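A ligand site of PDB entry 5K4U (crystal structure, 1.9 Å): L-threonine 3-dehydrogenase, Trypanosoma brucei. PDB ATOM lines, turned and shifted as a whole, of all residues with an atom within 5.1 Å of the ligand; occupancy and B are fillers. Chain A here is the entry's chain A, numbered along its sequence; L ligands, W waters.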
ATOM      1  N   GLY A   8     -14.754 -29.541 -16.281  1.00  0.00           N
ATOM      2  CA  GLY A   8     -14.070 -28.989 -15.079  1.00  0.00           C
ATOM      3  C   GLY A   8     -14.792 -29.311 -13.765  1.00  0.00           C
ATOM      4  O   GLY A   8     -14.825 -28.534 -12.861  1.00  0.00           O
ATOM      5  N   ALA A   9     -15.337 -30.529 -13.675  1.00  0.00           N
ATOM      6  CA  ALA A   9     -16.259 -30.922 -12.657  1.00  0.00           C
ATOM      7  C   ALA A   9     -15.755 -31.287 -11.260  1.00  0.00           C
ATOM      8  O   ALA A   9     -16.560 -31.398 -10.324  1.00  0.00           O
ATOM      9  CB  ALA A   9     -17.094 -32.072 -13.224  1.00  0.00           C
ATOM     10  N   LEU A  10     -14.454 -31.509 -11.098  1.00  0.00           N
ATOM     11  CA  LEU A  10     -13.901 -31.941  -9.819  1.00  0.00           C
ATOM     12  C   LEU A  10     -13.545 -30.800  -8.841  1.00  0.00           C
ATOM     13  O   LEU A  10     -13.146 -31.075  -7.686  1.00  0.00           O
ATOM     14  CB  LEU A  10     -12.601 -32.762 -10.105  1.00  0.00           C
ATOM     15  CG  LEU A  10     -12.816 -34.045 -10.889  1.00  0.00           C
ATOM     16  CD1 LEU A  10     -11.538 -34.869 -11.028  1.00  0.00           C
ATOM     17  CD2 LEU A  10     -13.912 -34.893 -10.293  1.00  0.00           C
ATOM     18  N   GLY A  11     -13.668 -29.533  -9.283  1.00  0.00           N
ATOM     19  CA  GLY A  11     -13.260 -28.413  -8.479  1.00  0.00           C
ATOM     20  C   GLY A  11     -14.359 -27.997  -7.560  1.00  0.00           C
ATOM     21  O   GLY A  11     -15.283 -28.774  -7.296  1.00  0.00           O
ATOM     22  N   GLN A  12     -14.240 -26.793  -7.021  1.00  0.00           N
ATOM     23  CA  GLN A  12     -15.113 -26.349  -5.927  1.00  0.00           C
ATOM     24  C   GLN A  12     -16.600 -26.347  -6.348  1.00  0.00           C
ATOM     25  O   GLN A  12     -17.449 -26.951  -5.652  1.00  0.00           O
ATOM     26  CB  GLN A  12     -14.686 -24.978  -5.442  1.00  0.00           C
ATOM     27  CG  GLN A  12     -15.416 -24.576  -4.160  1.00  0.00           C
ATOM     28  CD  GLN A  12     -15.330 -23.153  -3.806  1.00  0.00           C
ATOM     29  OE1 GLN A  12     -14.563 -22.335  -4.384  1.00  0.00           O
ATOM     30  NE2 GLN A  12     -16.141 -22.804  -2.882  1.00  0.00           N
ATOM     31  N   ILE A  13     -16.904 -25.611  -7.412  1.00  0.00           N
ATOM     32  CA  ILE A  13     -18.238 -25.555  -7.914  1.00  0.00           C
ATOM     33  C   ILE A  13     -18.747 -26.892  -8.495  1.00  0.00           C
ATOM     34  O   ILE A  13     -19.833 -27.361  -8.146  1.00  0.00           O
ATOM     35  CB  ILE A  13     -18.387 -24.389  -8.900  1.00  0.00           C
ATOM     36  CG1 ILE A  13     -18.155 -23.067  -8.120  1.00  0.00           C
ATOM     37  CG2 ILE A  13     -19.770 -24.416  -9.507  1.00  0.00           C
ATOM     38  CD1 ILE A  13     -18.102 -21.833  -8.951  1.00  0.00           C
ATOM     39  N   GLY A  14     -17.960 -27.466  -9.363  1.00  0.00           N
ATOM     40  CA  GLY A  14     -18.302 -28.683 -10.070  1.00  0.00           C
ATOM     41  C   GLY A  14     -18.602 -29.856  -9.128  1.00  0.00           C
ATOM     42  O   GLY A  14     -19.449 -30.666  -9.444  1.00  0.00           O
ATOM     43  N   ASP A  34     -13.204 -33.884 -16.251  1.00  0.00           N
ATOM     44  CA  ASP A  34     -12.147 -32.995 -15.736  1.00  0.00           C
ATOM     45  C   ASP A  34     -10.797 -33.505 -16.302  1.00  0.00           C
ATOM     46  O   ASP A  34     -10.646 -34.663 -16.743  1.00  0.00           O
ATOM     47  CB  ASP A  34     -12.157 -32.996 -14.203  1.00  0.00           C
ATOM     48  CG  ASP A  34     -11.436 -31.813 -13.599  1.00  0.00           C
ATOM     49  OD1 ASP A  34     -10.151 -31.778 -13.628  1.00  0.00           O
ATOM     50  OD2 ASP A  34     -12.102 -30.963 -12.964  1.00  0.00           O
ATOM     51  N   VAL A  35      -9.860 -32.591 -16.414  1.00  0.00           N
ATOM     52  CA  VAL A  35      -8.537 -32.892 -16.895  1.00  0.00           C
ATOM     53  C   VAL A  35      -7.810 -33.893 -16.007  1.00  0.00           C
ATOM     54  O   VAL A  35      -6.972 -34.611 -16.528  1.00  0.00           O
ATOM     55  CB  VAL A  35      -7.747 -31.590 -17.128  1.00  0.00           C
ATOM     56  CG1 VAL A  35      -7.404 -30.874 -15.847  1.00  0.00           C
ATOM     57  CG2 VAL A  35      -6.495 -31.839 -17.971  1.00  0.00           C
ATOM     58  N   VAL A  36      -8.111 -33.905 -14.690  1.00  0.00           N
ATOM     59  CA  VAL A  36      -7.579 -34.905 -13.742  1.00  0.00           C
ATOM     60  C   VAL A  36      -8.634 -36.010 -13.387  1.00  0.00           C
ATOM     61  O   VAL A  36      -9.851 -35.809 -13.534  1.00  0.00           O
ATOM     62  CB  VAL A  36      -6.909 -34.193 -12.503  1.00  0.00           C
ATOM     63  CG1 VAL A  36      -5.855 -33.147 -12.973  1.00  0.00           C
ATOM     64  CG2 VAL A  36      -7.874 -33.473 -11.599  1.00  0.00           C
ATOM     65  N   LEU A  53     -11.050 -35.709 -19.334  1.00  0.00           N
ATOM     66  CA  LEU A  53     -11.066 -35.002 -20.603  1.00  0.00           C
ATOM     67  C   LEU A  53     -10.345 -33.672 -20.328  1.00  0.00           C
ATOM     68  O   LEU A  53     -10.784 -32.890 -19.478  1.00  0.00           O
ATOM     69  CB  LEU A  53     -12.479 -34.712 -21.080  1.00  0.00           C
ATOM     70  CG  LEU A  53     -12.584 -33.617 -22.162  1.00  0.00           C
ATOM     71  CD1 LEU A  53     -11.972 -34.093 -23.466  1.00  0.00           C
ATOM     72  CD2 LEU A  53     -13.985 -33.156 -22.406  1.00  0.00           C
ATOM     73  N   ASP A  54      -9.316 -33.393 -21.108  1.00  0.00           N
ATOM     74  CA  ASP A  54      -8.703 -32.079 -21.189  1.00  0.00           C
ATOM     75  C   ASP A  54      -9.497 -31.252 -22.219  1.00  0.00           C
ATOM     76  O   ASP A  54      -9.529 -31.595 -23.392  1.00  0.00           O
ATOM     77  CB  ASP A  54      -7.288 -32.181 -21.682  1.00  0.00           C
ATOM     78  CG  ASP A  54      -6.515 -30.865 -21.594  1.00  0.00           C
ATOM     79  OD1 ASP A  54      -7.092 -29.748 -21.599  1.00  0.00           O
ATOM     80  OD2 ASP A  54      -5.293 -30.944 -21.514  1.00  0.00           O
ATOM     81  N   CYS A  55     -10.136 -30.164 -21.774  1.00  0.00           N
ATOM     82  CA  CYS A  55     -10.932 -29.362 -22.698  1.00  0.00           C
ATOM     83  C   CYS A  55     -10.056 -28.643 -23.770  1.00  0.00           C
ATOM     84  O   CYS A  55     -10.580 -28.134 -24.752  1.00  0.00           O
ATOM     85  CB  CYS A  55     -11.772 -28.384 -21.910  1.00  0.00           C
ATOM     86  SG  CYS A  55     -13.242 -29.173 -21.182  1.00  0.00           S
ATOM     87  N   LEU A  56      -8.746 -28.537 -23.567  1.00  0.00           N
ATOM     88  CA  LEU A  56      -7.870 -27.985 -24.602  1.00  0.00           C
ATOM     89  C   LEU A  56      -7.631 -28.998 -25.726  1.00  0.00           C
ATOM     90  O   LEU A  56      -7.070 -28.636 -26.726  1.00  0.00           O
ATOM     91  CB  LEU A  56      -6.504 -27.544 -24.054  1.00  0.00           C
ATOM     92  CG  LEU A  56      -6.523 -26.242 -23.274  1.00  0.00           C
ATOM     93  CD1 LEU A  56      -5.115 -25.971 -22.761  1.00  0.00           C
ATOM     94  CD2 LEU A  56      -6.970 -25.138 -24.209  1.00  0.00           C
ATOM     95  N   HIS A  75     -19.801 -25.259 -18.359  1.00  0.00           N
ATOM     96  CA  HIS A  75     -18.411 -25.313 -18.743  1.00  0.00           C
ATOM     97  C   HIS A  75     -17.646 -24.534 -17.697  1.00  0.00           C
ATOM     98  O   HIS A  75     -17.674 -23.290 -17.699  1.00  0.00           O
ATOM     99  CB  HIS A  75     -18.200 -24.716 -20.139  1.00  0.00           C
ATOM    100  CG  HIS A  75     -16.800 -24.690 -20.531  1.00  0.00           C
ATOM    101  ND1 HIS A  75     -16.119 -25.856 -20.816  1.00  0.00           N
ATOM    102  CD2 HIS A  75     -15.889 -23.691 -20.555  1.00  0.00           C
ATOM    103  CE1 HIS A  75     -14.864 -25.550 -21.044  1.00  0.00           C
ATOM    104  NE2 HIS A  75     -14.701 -24.245 -20.926  1.00  0.00           N
ATOM    105  N   LEU A  76     -16.971 -25.277 -16.802  1.00  0.00           N
ATOM    106  CA  LEU A  76     -16.364 -24.682 -15.598  1.00  0.00           C
ATOM    107  C   LEU A  76     -14.894 -24.459 -15.578  1.00  0.00           C
ATOM    108  O   LEU A  76     -14.413 -23.670 -14.730  1.00  0.00           O
ATOM    109  CB  LEU A  76     -16.786 -25.464 -14.327  1.00  0.00           C
ATOM    110  CG  LEU A  76     -18.268 -25.820 -14.136  1.00  0.00           C
ATOM    111  CD1 LEU A  76     -18.487 -26.567 -12.844  1.00  0.00           C
ATOM    112  CD2 LEU A  76     -19.109 -24.559 -14.114  1.00  0.00           C
ATOM    113  N   PRO A  77     -14.122 -25.071 -16.496  1.00  0.00           N
ATOM    114  CA  PRO A  77     -12.710 -24.831 -16.226  1.00  0.00           C
ATOM    115  C   PRO A  77     -12.227 -23.417 -16.474  1.00  0.00           C
ATOM    116  O   PRO A  77     -12.534 -22.840 -17.505  1.00  0.00           O
ATOM    117  CB  PRO A  77     -12.003 -25.836 -17.156  1.00  0.00           C
ATOM    118  CG  PRO A  77     -12.914 -25.988 -18.270  1.00  0.00           C
ATOM    119  CD  PRO A  77     -14.323 -25.931 -17.673  1.00  0.00           C
ATOM    120  N   ALA A  78     -11.425 -22.903 -15.548  1.00  0.00           N
ATOM    121  CA  ALA A  78     -10.714 -21.608 -15.676  1.00  0.00           C
ATOM    122  C   ALA A  78      -9.673 -21.520 -14.606  1.00  0.00           C
ATOM    123  O   ALA A  78      -9.827 -22.106 -13.557  1.00  0.00           O
ATOM    124  CB  ALA A  78     -11.614 -20.387 -15.565  1.00  0.00           C
ATOM    125  N   MET A  80      -8.168 -18.988 -12.019  1.00  0.00           N
ATOM    126  CA  MET A  80      -8.850 -17.894 -11.360  1.00  0.00           C
ATOM    127  C   MET A  80      -7.889 -16.746 -10.988  1.00  0.00           C
ATOM    128  O   MET A  80      -6.723 -16.679 -11.468  1.00  0.00           O
ATOM    129  CB  MET A  80      -9.718 -18.457 -10.197  1.00  0.00           C
ATOM    130  CG  MET A  80     -10.847 -19.354 -10.725  1.00  0.00           C
ATOM    131  SD  MET A  80     -11.934 -19.868  -9.447  1.00  0.00           S
ATOM    132  CE  MET A  80     -10.876 -21.030  -8.599  1.00  0.00           C
ATOM    133  N   ILE A  94      -6.128 -21.661 -21.090  1.00  0.00           N
ATOM    134  CA  ILE A  94      -7.393 -22.340 -20.627  1.00  0.00           C
ATOM    135  C   ILE A  94      -8.652 -21.496 -20.785  1.00  0.00           C
ATOM    136  O   ILE A  94      -9.694 -21.945 -21.354  1.00  0.00           O
ATOM    137  CB  ILE A  94      -7.295 -22.822 -19.138  1.00  0.00           C
ATOM    138  CG1 ILE A  94      -6.139 -23.843 -18.824  1.00  0.00           C
ATOM    139  CG2 ILE A  94      -8.573 -23.503 -18.668  1.00  0.00           C
ATOM    140  CD1 ILE A  94      -6.103 -25.051 -19.669  1.00  0.00           C
ATOM    141  N   THR A  98     -10.439 -23.103 -24.139  1.00  0.00           N
ATOM    142  CA  THR A  98     -11.503 -24.095 -23.777  1.00  0.00           C
ATOM    143  C   THR A  98     -12.930 -23.459 -24.015  1.00  0.00           C
ATOM    144  O   THR A  98     -13.883 -24.138 -24.419  1.00  0.00           O
ATOM    145  CB  THR A  98     -11.377 -24.647 -22.368  1.00  0.00           C
ATOM    146  OG1 THR A  98     -11.730 -23.668 -21.365  1.00  0.00           O
ATOM    147  CG2 THR A  98      -9.992 -25.230 -22.105  1.00  0.00           C
ATOM    148  N   PRO A 116     -19.786 -19.597 -16.460  1.00  0.00           N
ATOM    149  CA  PRO A 116     -19.780 -18.604 -15.428  1.00  0.00           C
ATOM    150  C   PRO A 116     -18.826 -17.444 -15.702  1.00  0.00           C
ATOM    151  O   PRO A 116     -17.691 -17.669 -16.198  1.00  0.00           O
ATOM    152  CB  PRO A 116     -19.339 -19.370 -14.171  1.00  0.00           C
ATOM    153  CG  PRO A 116     -18.719 -20.649 -14.646  1.00  0.00           C
ATOM    154  CD  PRO A 116     -19.227 -20.897 -16.034  1.00  0.00           C
ATOM    155  N   SER A 117     -19.294 -16.231 -15.406  1.00  0.00           N
ATOM    156  CA  SER A 117     -18.436 -15.096 -15.279  1.00  0.00           C
ATOM    157  C   SER A 117     -18.178 -14.896 -13.793  1.00  0.00           C
ATOM    158  O   SER A 117     -18.382 -15.832 -12.993  1.00  0.00           O
ATOM    159  CB  SER A 117     -19.010 -13.903 -16.000  1.00  0.00           C
ATOM    160  OG  SER A 117     -17.989 -12.936 -16.139  1.00  0.00           O
ATOM    161  N   THR A 118     -17.744 -13.688 -13.402  1.00  0.00           N
ATOM    162  CA  THR A 118     -17.239 -13.457 -12.109  1.00  0.00           C
ATOM    163  C   THR A 118     -17.236 -11.989 -11.821  1.00  0.00           C
ATOM    164  O   THR A 118     -17.130 -11.188 -12.751  1.00  0.00           O
ATOM    165  CB  THR A 118     -15.799 -13.988 -11.984  1.00  0.00           C
ATOM    166  OG1 THR A 118     -15.276 -13.582 -10.723  1.00  0.00           O
ATOM    167  CG2 THR A 118     -14.885 -13.495 -13.111  1.00  0.00           C
ATOM    168  N   TYR A 143      -7.249 -12.929 -15.499  1.00  0.00           N
ATOM    169  CA  TYR A 143      -8.468 -13.713 -15.353  1.00  0.00           C
ATOM    170  C   TYR A 143      -9.658 -12.876 -15.694  1.00  0.00           C
ATOM    171  O   TYR A 143     -10.538 -13.296 -16.520  1.00  0.00           O
ATOM    172  CB  TYR A 143      -8.579 -14.183 -13.956  1.00  0.00           C
ATOM    173  CG  TYR A 143      -9.887 -14.761 -13.461  1.00  0.00           C
ATOM    174  CD1 TYR A 143     -10.454 -15.920 -14.003  1.00  0.00           C
ATOM    175  CD2 TYR A 143     -10.462 -14.227 -12.325  1.00  0.00           C
ATOM    176  CE1 TYR A 143     -11.624 -16.463 -13.488  1.00  0.00           C
ATOM    177  CE2 TYR A 143     -11.606 -14.801 -11.769  1.00  0.00           C
ATOM    178  CZ  TYR A 143     -12.161 -15.928 -12.327  1.00  0.00           C
ATOM    179  OH  TYR A 143     -13.297 -16.532 -11.794  1.00  0.00           O
ATOM    180  N   LYS A 147     -12.431 -13.273 -18.701  1.00  0.00           N
ATOM    181  CA  LYS A 147     -13.870 -13.404 -18.415  1.00  0.00           C
ATOM    182  C   LYS A 147     -14.721 -12.342 -19.136  1.00  0.00           C
ATOM    183  O   LYS A 147     -15.867 -12.614 -19.518  1.00  0.00           O
ATOM    184  CB  LYS A 147     -14.128 -13.467 -16.902  1.00  0.00           C
ATOM    185  CG  LYS A 147     -13.587 -14.737 -16.227  1.00  0.00           C
ATOM    186  CD  LYS A 147     -14.337 -15.963 -16.719  1.00  0.00           C
ATOM    187  CE  LYS A 147     -14.084 -17.168 -15.860  1.00  0.00           C
ATOM    188  NZ  LYS A 147     -14.910 -18.300 -16.308  1.00  0.00           N
ATOM    189  N   LEU A 170     -20.617 -14.717 -10.885  1.00  0.00           N
ATOM    190  CA  LEU A 170     -20.593 -15.290  -9.575  1.00  0.00           C
ATOM    191  C   LEU A 170     -19.742 -14.403  -8.672  1.00  0.00           C
ATOM    192  O   LEU A 170     -18.676 -13.952  -9.045  1.00  0.00           O
ATOM    193  CB  LEU A 170     -19.987 -16.710  -9.584  1.00  0.00           C
ATOM    194  CG  LEU A 170     -20.835 -17.767 -10.271  1.00  0.00           C
ATOM    195  CD1 LEU A 170     -20.125 -19.086 -10.292  1.00  0.00           C
ATOM    196  CD2 LEU A 170     -22.077 -18.011  -9.470  1.00  0.00           C
ATOM    197  N   PRO A 171     -20.218 -14.214  -7.434  1.00  0.00           N
ATOM    198  CA  PRO A 171     -19.488 -13.619  -6.360  1.00  0.00           C
ATOM    199  C   PRO A 171     -18.543 -14.650  -5.757  1.00  0.00           C
ATOM    200  O   PRO A 171     -18.479 -15.730  -6.264  1.00  0.00           O
ATOM    201  CB  PRO A 171     -20.641 -13.282  -5.394  1.00  0.00           C
ATOM    202  CG  PRO A 171     -21.580 -14.387  -5.571  1.00  0.00           C
ATOM    203  CD  PRO A 171     -21.534 -14.734  -7.013  1.00  0.00           C
ATOM    204  N   GLY A 172     -17.807 -14.334  -4.700  1.00  0.00           N
ATOM    205  CA  GLY A 172     -17.062 -15.413  -4.015  1.00  0.00           C
ATOM    206  C   GLY A 172     -18.030 -16.528  -3.537  1.00  0.00           C
ATOM    207  O   GLY A 172     -19.045 -16.252  -2.889  1.00  0.00           O
ATOM    208  N   ILE A 173     -17.712 -17.788  -3.820  1.00  0.00           N
ATOM    209  CA  ILE A 173     -18.561 -18.879  -3.415  1.00  0.00           C
ATOM    210  C   ILE A 173     -17.886 -19.621  -2.245  1.00  0.00           C
ATOM    211  O   ILE A 173     -16.642 -19.870  -2.262  1.00  0.00           O
ATOM    212  CB  ILE A 173     -18.834 -19.861  -4.573  1.00  0.00           C
ATOM    213  CG1 ILE A 173     -19.389 -19.126  -5.808  1.00  0.00           C
ATOM    214  CG2 ILE A 173     -19.811 -20.937  -4.132  1.00  0.00           C
ATOM    215  CD1 ILE A 173     -20.683 -18.362  -5.580  1.00  0.00           C
ATOM    216  N   LEU A 179     -11.935 -28.027  -1.600  1.00  0.00           N
ATOM    217  CA  LEU A 179     -11.119 -26.837  -1.360  1.00  0.00           C
ATOM    218  C   LEU A 179     -11.016 -25.950  -2.625  1.00  0.00           C
ATOM    219  O   LEU A 179     -10.913 -26.435  -3.763  1.00  0.00           O
ATOM    220  CB  LEU A 179      -9.753 -27.230  -0.816  1.00  0.00           C
ATOM    221  CG  LEU A 179      -9.730 -27.843   0.617  1.00  0.00           C
ATOM    222  CD1 LEU A 179      -8.324 -28.309   0.898  1.00  0.00           C
ATOM    223  CD2 LEU A 179     -10.124 -26.915   1.751  1.00  0.00           C
ATOM    224  N   PRO A 180     -10.971 -24.622  -2.436  1.00  0.00           N
ATOM    225  CA  PRO A 180     -11.063 -23.682  -3.601  1.00  0.00           C
ATOM    226  C   PRO A 180      -9.803 -23.661  -4.430  1.00  0.00           C
ATOM    227  O   PRO A 180      -8.768 -24.220  -3.973  1.00  0.00           O
ATOM    228  CB  PRO A 180     -11.302 -22.339  -2.914  1.00  0.00           C
ATOM    229  CG  PRO A 180     -10.663 -22.469  -1.589  1.00  0.00           C
ATOM    230  CD  PRO A 180     -11.009 -23.884  -1.159  1.00  0.00           C
ATOM    231  N   GLY A 181      -9.885 -23.147  -5.668  1.00  0.00           N
ATOM    232  CA  GLY A 181      -8.756 -23.274  -6.604  1.00  0.00           C
ATOM    233  C   GLY A 181      -7.811 -22.091  -6.789  1.00  0.00           C
ATOM    234  O   GLY A 181      -7.110 -22.028  -7.806  1.00  0.00           O
ATOM    235  N   THR A 185     -11.002 -14.702  -2.999  1.00  0.00           N
ATOM    236  CA  THR A 185     -11.982 -14.993  -1.933  1.00  0.00           C
ATOM    237  C   THR A 185     -11.731 -16.334  -1.180  1.00  0.00           C
ATOM    238  O   THR A 185     -12.458 -16.603  -0.225  1.00  0.00           O
ATOM    239  CB  THR A 185     -13.432 -15.025  -2.442  1.00  0.00           C
ATOM    240  OG1 THR A 185     -13.590 -16.080  -3.381  1.00  0.00           O
ATOM    241  CG2 THR A 185     -13.845 -13.744  -3.062  1.00  0.00           C
HETATM  242  P1  LIG L   1     -11.670 -24.892  -9.326  1.00  0.00           P
HETATM  243  O1  LIG L   1     -12.011 -25.353  -7.929  1.00  0.00           O
HETATM  244  O2  LIG L   1     -10.357 -24.403  -9.628  1.00  0.00           O
HETATM  245  O3  LIG L   1     -11.937 -26.007 -10.399  1.00  0.00           O
HETATM  246  C1  LIG L   1     -11.497 -26.011 -11.791  1.00  0.00           C
HETATM  247  C2  LIG L   1     -11.660 -27.390 -12.330  1.00  0.00           C
HETATM  248  O4  LIG L   1     -11.297 -27.249 -13.771  1.00  0.00           O
HETATM  249  C3  LIG L   1     -10.589 -28.244 -11.654  1.00  0.00           C
HETATM  250  O5  LIG L   1     -11.085 -29.524 -11.185  1.00  0.00           O
HETATM  251  C4  LIG L   1      -9.544 -28.403 -12.788  1.00  0.00           C
HETATM  252  O6  LIG L   1      -8.864 -29.654 -12.674  1.00  0.00           O
HETATM  253  C5  LIG L   1     -10.440 -28.337 -14.047  1.00  0.00           C
HETATM  254  N1  LIG L   1      -9.659 -28.017 -15.228  1.00  0.00           N
HETATM  255  C6  LIG L   1      -8.618 -27.149 -15.265  1.00  0.00           C
HETATM  256  N2  LIG L   1      -8.153 -27.102 -16.531  1.00  0.00           N
HETATM  257  C7  LIG L   1      -8.884 -27.945 -17.269  1.00  0.00           C
HETATM  258  C8  LIG L   1      -8.860 -28.308 -18.592  1.00  0.00           C
HETATM  259  N3  LIG L   1      -7.999 -27.802 -19.477  1.00  0.00           N
HETATM  260  N4  LIG L   1      -9.805 -29.172 -19.007  1.00  0.00           N
HETATM  261  C9  LIG L   1     -10.718 -29.672 -18.198  1.00  0.00           C
HETATM  262  N5  LIG L   1     -10.802 -29.398 -16.927  1.00  0.00           N
HETATM  263  C10 LIG L   1      -9.871 -28.512 -16.447  1.00  0.00           C
HETATM  264  O7  LIG L   1     -12.691 -23.706  -9.769  1.00  0.00           O
HETATM  265  P2  LIG L   1     -14.242 -23.477  -9.374  1.00  0.00           P
HETATM  266  O8  LIG L   1     -14.997 -24.774  -9.295  1.00  0.00           O
HETATM  267  O9  LIG L   1     -14.030 -22.621  -8.192  1.00  0.00           O
HETATM  268  O10 LIG L   1     -14.591 -22.530 -10.603  1.00  0.00           O
HETATM  269  C11 LIG L   1     -15.385 -23.036 -11.627  1.00  0.00           C
HETATM  270  C12 LIG L   1     -15.764 -21.834 -12.521  1.00  0.00           C
HETATM  271  O11 LIG L   1     -16.577 -20.874 -11.718  1.00  0.00           O
HETATM  272  C13 LIG L   1     -14.717 -21.046 -13.218  1.00  0.00           C
HETATM  273  O12 LIG L   1     -15.193 -20.620 -14.523  1.00  0.00           O
HETATM  274  C14 LIG L   1     -14.502 -19.863 -12.294  1.00  0.00           C
HETATM  275  O13 LIG L   1     -14.027 -18.726 -13.007  1.00  0.00           O
HETATM  276  C15 LIG L   1     -15.932 -19.626 -11.901  1.00  0.00           C
HETATM  277  N6  LIG L   1     -16.074 -18.857 -10.627  1.00  0.00           N
HETATM  278  C16 LIG L   1     -15.806 -19.416  -9.328  1.00  0.00           C
HETATM  279  C17 LIG L   1     -15.904 -18.621  -8.190  1.00  0.00           C
HETATM  280  C18 LIG L   1     -15.631 -19.240  -6.795  1.00  0.00           C
HETATM  281  O14 LIG L   1     -15.814 -18.457  -5.750  1.00  0.00           O
HETATM  282  N7  LIG L   1     -15.333 -20.599  -6.670  1.00  0.00           N
HETATM  283  C19 LIG L   1     -16.320 -17.272  -8.322  1.00  0.00           C
HETATM  284  C20 LIG L   1     -16.576 -16.724  -9.601  1.00  0.00           C
HETATM  285  C21 LIG L   1     -16.487 -17.487 -10.764  1.00  0.00           C
HETATM  286  O   HOH W   1     -10.416 -26.521  -6.216  1.00  0.00           O
HETATM  287  O   HOH W   2      -7.562 -25.685 -12.341  1.00  0.00           O
HETATM  288  O   HOH W   3     -12.511 -22.322  -6.098  1.00  0.00           O
HETATM  289  O   HOH W   4     -13.389 -31.661 -18.989  1.00  0.00           O
HETATM  290  O   HOH W   5     -15.347 -21.638 -17.040  1.00  0.00           O
HETATM  291  O   HOH W   6     -15.282 -27.083 -10.453  1.00  0.00           O
HETATM  292  O   HOH W   7      -8.759 -23.192 -11.501  1.00  0.00           O
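Water W6 lies within hydrogen-bond range of O8 of the ligand, O of Gly 8, N of Gly 14 and N of Gly 11.
Water W3 lies within hydrogen-bond range of O9 of the ligand (2.6 Å), OE1 of Gln 12 (2.7 Å) and N of Gly 181 (2.8 Å).
Water W1 lies within hydrogen-bond range of O of Leu 179, O1 of the ligand and N of Gly 181.
Water W7 bridges O of Ala 78 and O2 of the ligand.
Water W4 bridges O of Leu 53 (2.9 Å) and SG of Cys 55 (3.3 Å).
The side-chain hydroxyl (OH) of Tyr 143 lies within hydrogen-bond range of an oxygen (O13) of the ligand (2.6 Å).
The backbone NH of Gln 12 sits at hydrogen-bond distance from an oxygen (O1) of the ligand, at 2.8 Å.
O14 of the ligand is in hydrogen-bond range of N of Ile 173 (2.8 Å).
The backbone NH of Val 35 sits at hydrogen-bond distance from a nitrogen (N5) of the ligand, at 3.4 Å.
O5 of the ligand sits at hydrogen-bond distance from N of Gly 11, at 3.2 Å.
The side-chain carboxylate (OD1) of Asp 54 lies within hydrogen-bond range of a nitrogen (N3) of the ligand (3.0 Å).
O8 of the ligand sits at hydrogen-bond distance from N of Ile 13, 2.8 Å away.
A nitrogen (N7) of the ligand is in hydrogen-bond range of the side-chain amide oxygen of Gln 12 (3.0 Å).
The side-chain amino group (NZ) of Lys 147 sits at hydrogen-bond distance from an oxygen (O12) of the ligand (2.9 Å).
The backbone NH of Cys 55 sits at hydrogen-bond distance from a nitrogen (N4) of the ligand (3.0 Å).
OD2 of Asp 34 sits at hydrogen-bond distance from O5 of the ligand, at 2.5 Å.
O of Leu 76 lies close to O12 of the ligand (3.2 Å).
An oxygen (O9) of the ligand lies close to the side-chain sulfur of Met 80.
Gly 8 touches the ligand (O to C2, 3.4 Å).
Leu 10 touches the ligand (C to O5, 3.6 Å).
O of Leu 53 touches C9 of the ligand (3.5 Å).
Pro 77 touches the ligand.
Ala 78 touches the ligand.
CD1 of Ile 94 touches N3 of the ligand, at 3.3 Å.
Pro 116 touches the ligand (CG to O12, 3.5 Å).
O of Ser 117 touches C21 of the ligand, at 3.4 Å.
OG1 of Thr 118 touches C20 of the ligand (3.6 Å).
Leu 170 touches the ligand (CB to C20, 3.4 Å).
Pro 171 touches the ligand.
C of Gly 172 touches O14 of the ligand, at 3.7 Å.
Gly 181 touches the ligand (CA to O2, 3.6 Å).
Hydrophobic or aromatic side chains that line the ligand: Leu 10, Ile 13, Val 35, Leu 76, Pro 77, Ala 78, Met 80, Ile 94, Pro 116, Tyr 143, Leu 170 and Ile 173.
Of the 34 residues printed, 25 come within 4 Å of the ligand.
The nearest printed residue that does not touch the ligand is Gly 14 (4.004 Å).
The backbone carbonyl oxygen (O) of Pro 116 lies within hydrogen-bond range of the side-chain amino group (NZ) of Lys 147, at 2.9 Å.
O of Asp 34 sits at hydrogen-bond distance from N of Leu 53 (2.8 Å).
The backbone carbonyl oxygen (O) of Ile 94 sits at hydrogen-bond distance from the side-chain hydroxyl (OG1) of Thr 98.
OD1 of Asp 34 lies within hydrogen-bond range of N of Val 36 (3.1 Å).
OD1 of Asp 54 is in hydrogen-bond range of N of Leu 56, 2.8 Å away.
The backbone carbonyl oxygen (O) of Ile 173 lies within hydrogen-bond range of the side-chain amide nitrogen (NE2) of Gln 12, 3.0 Å away.
The side-chain carboxylate (OD2) of Asp 34 is in hydrogen-bond range of the backbone NH (N) of Ala 9, at 3.3 Å.
OD2 of Asp 34 lies within hydrogen-bond range of N of Leu 10, at 3.1 Å.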
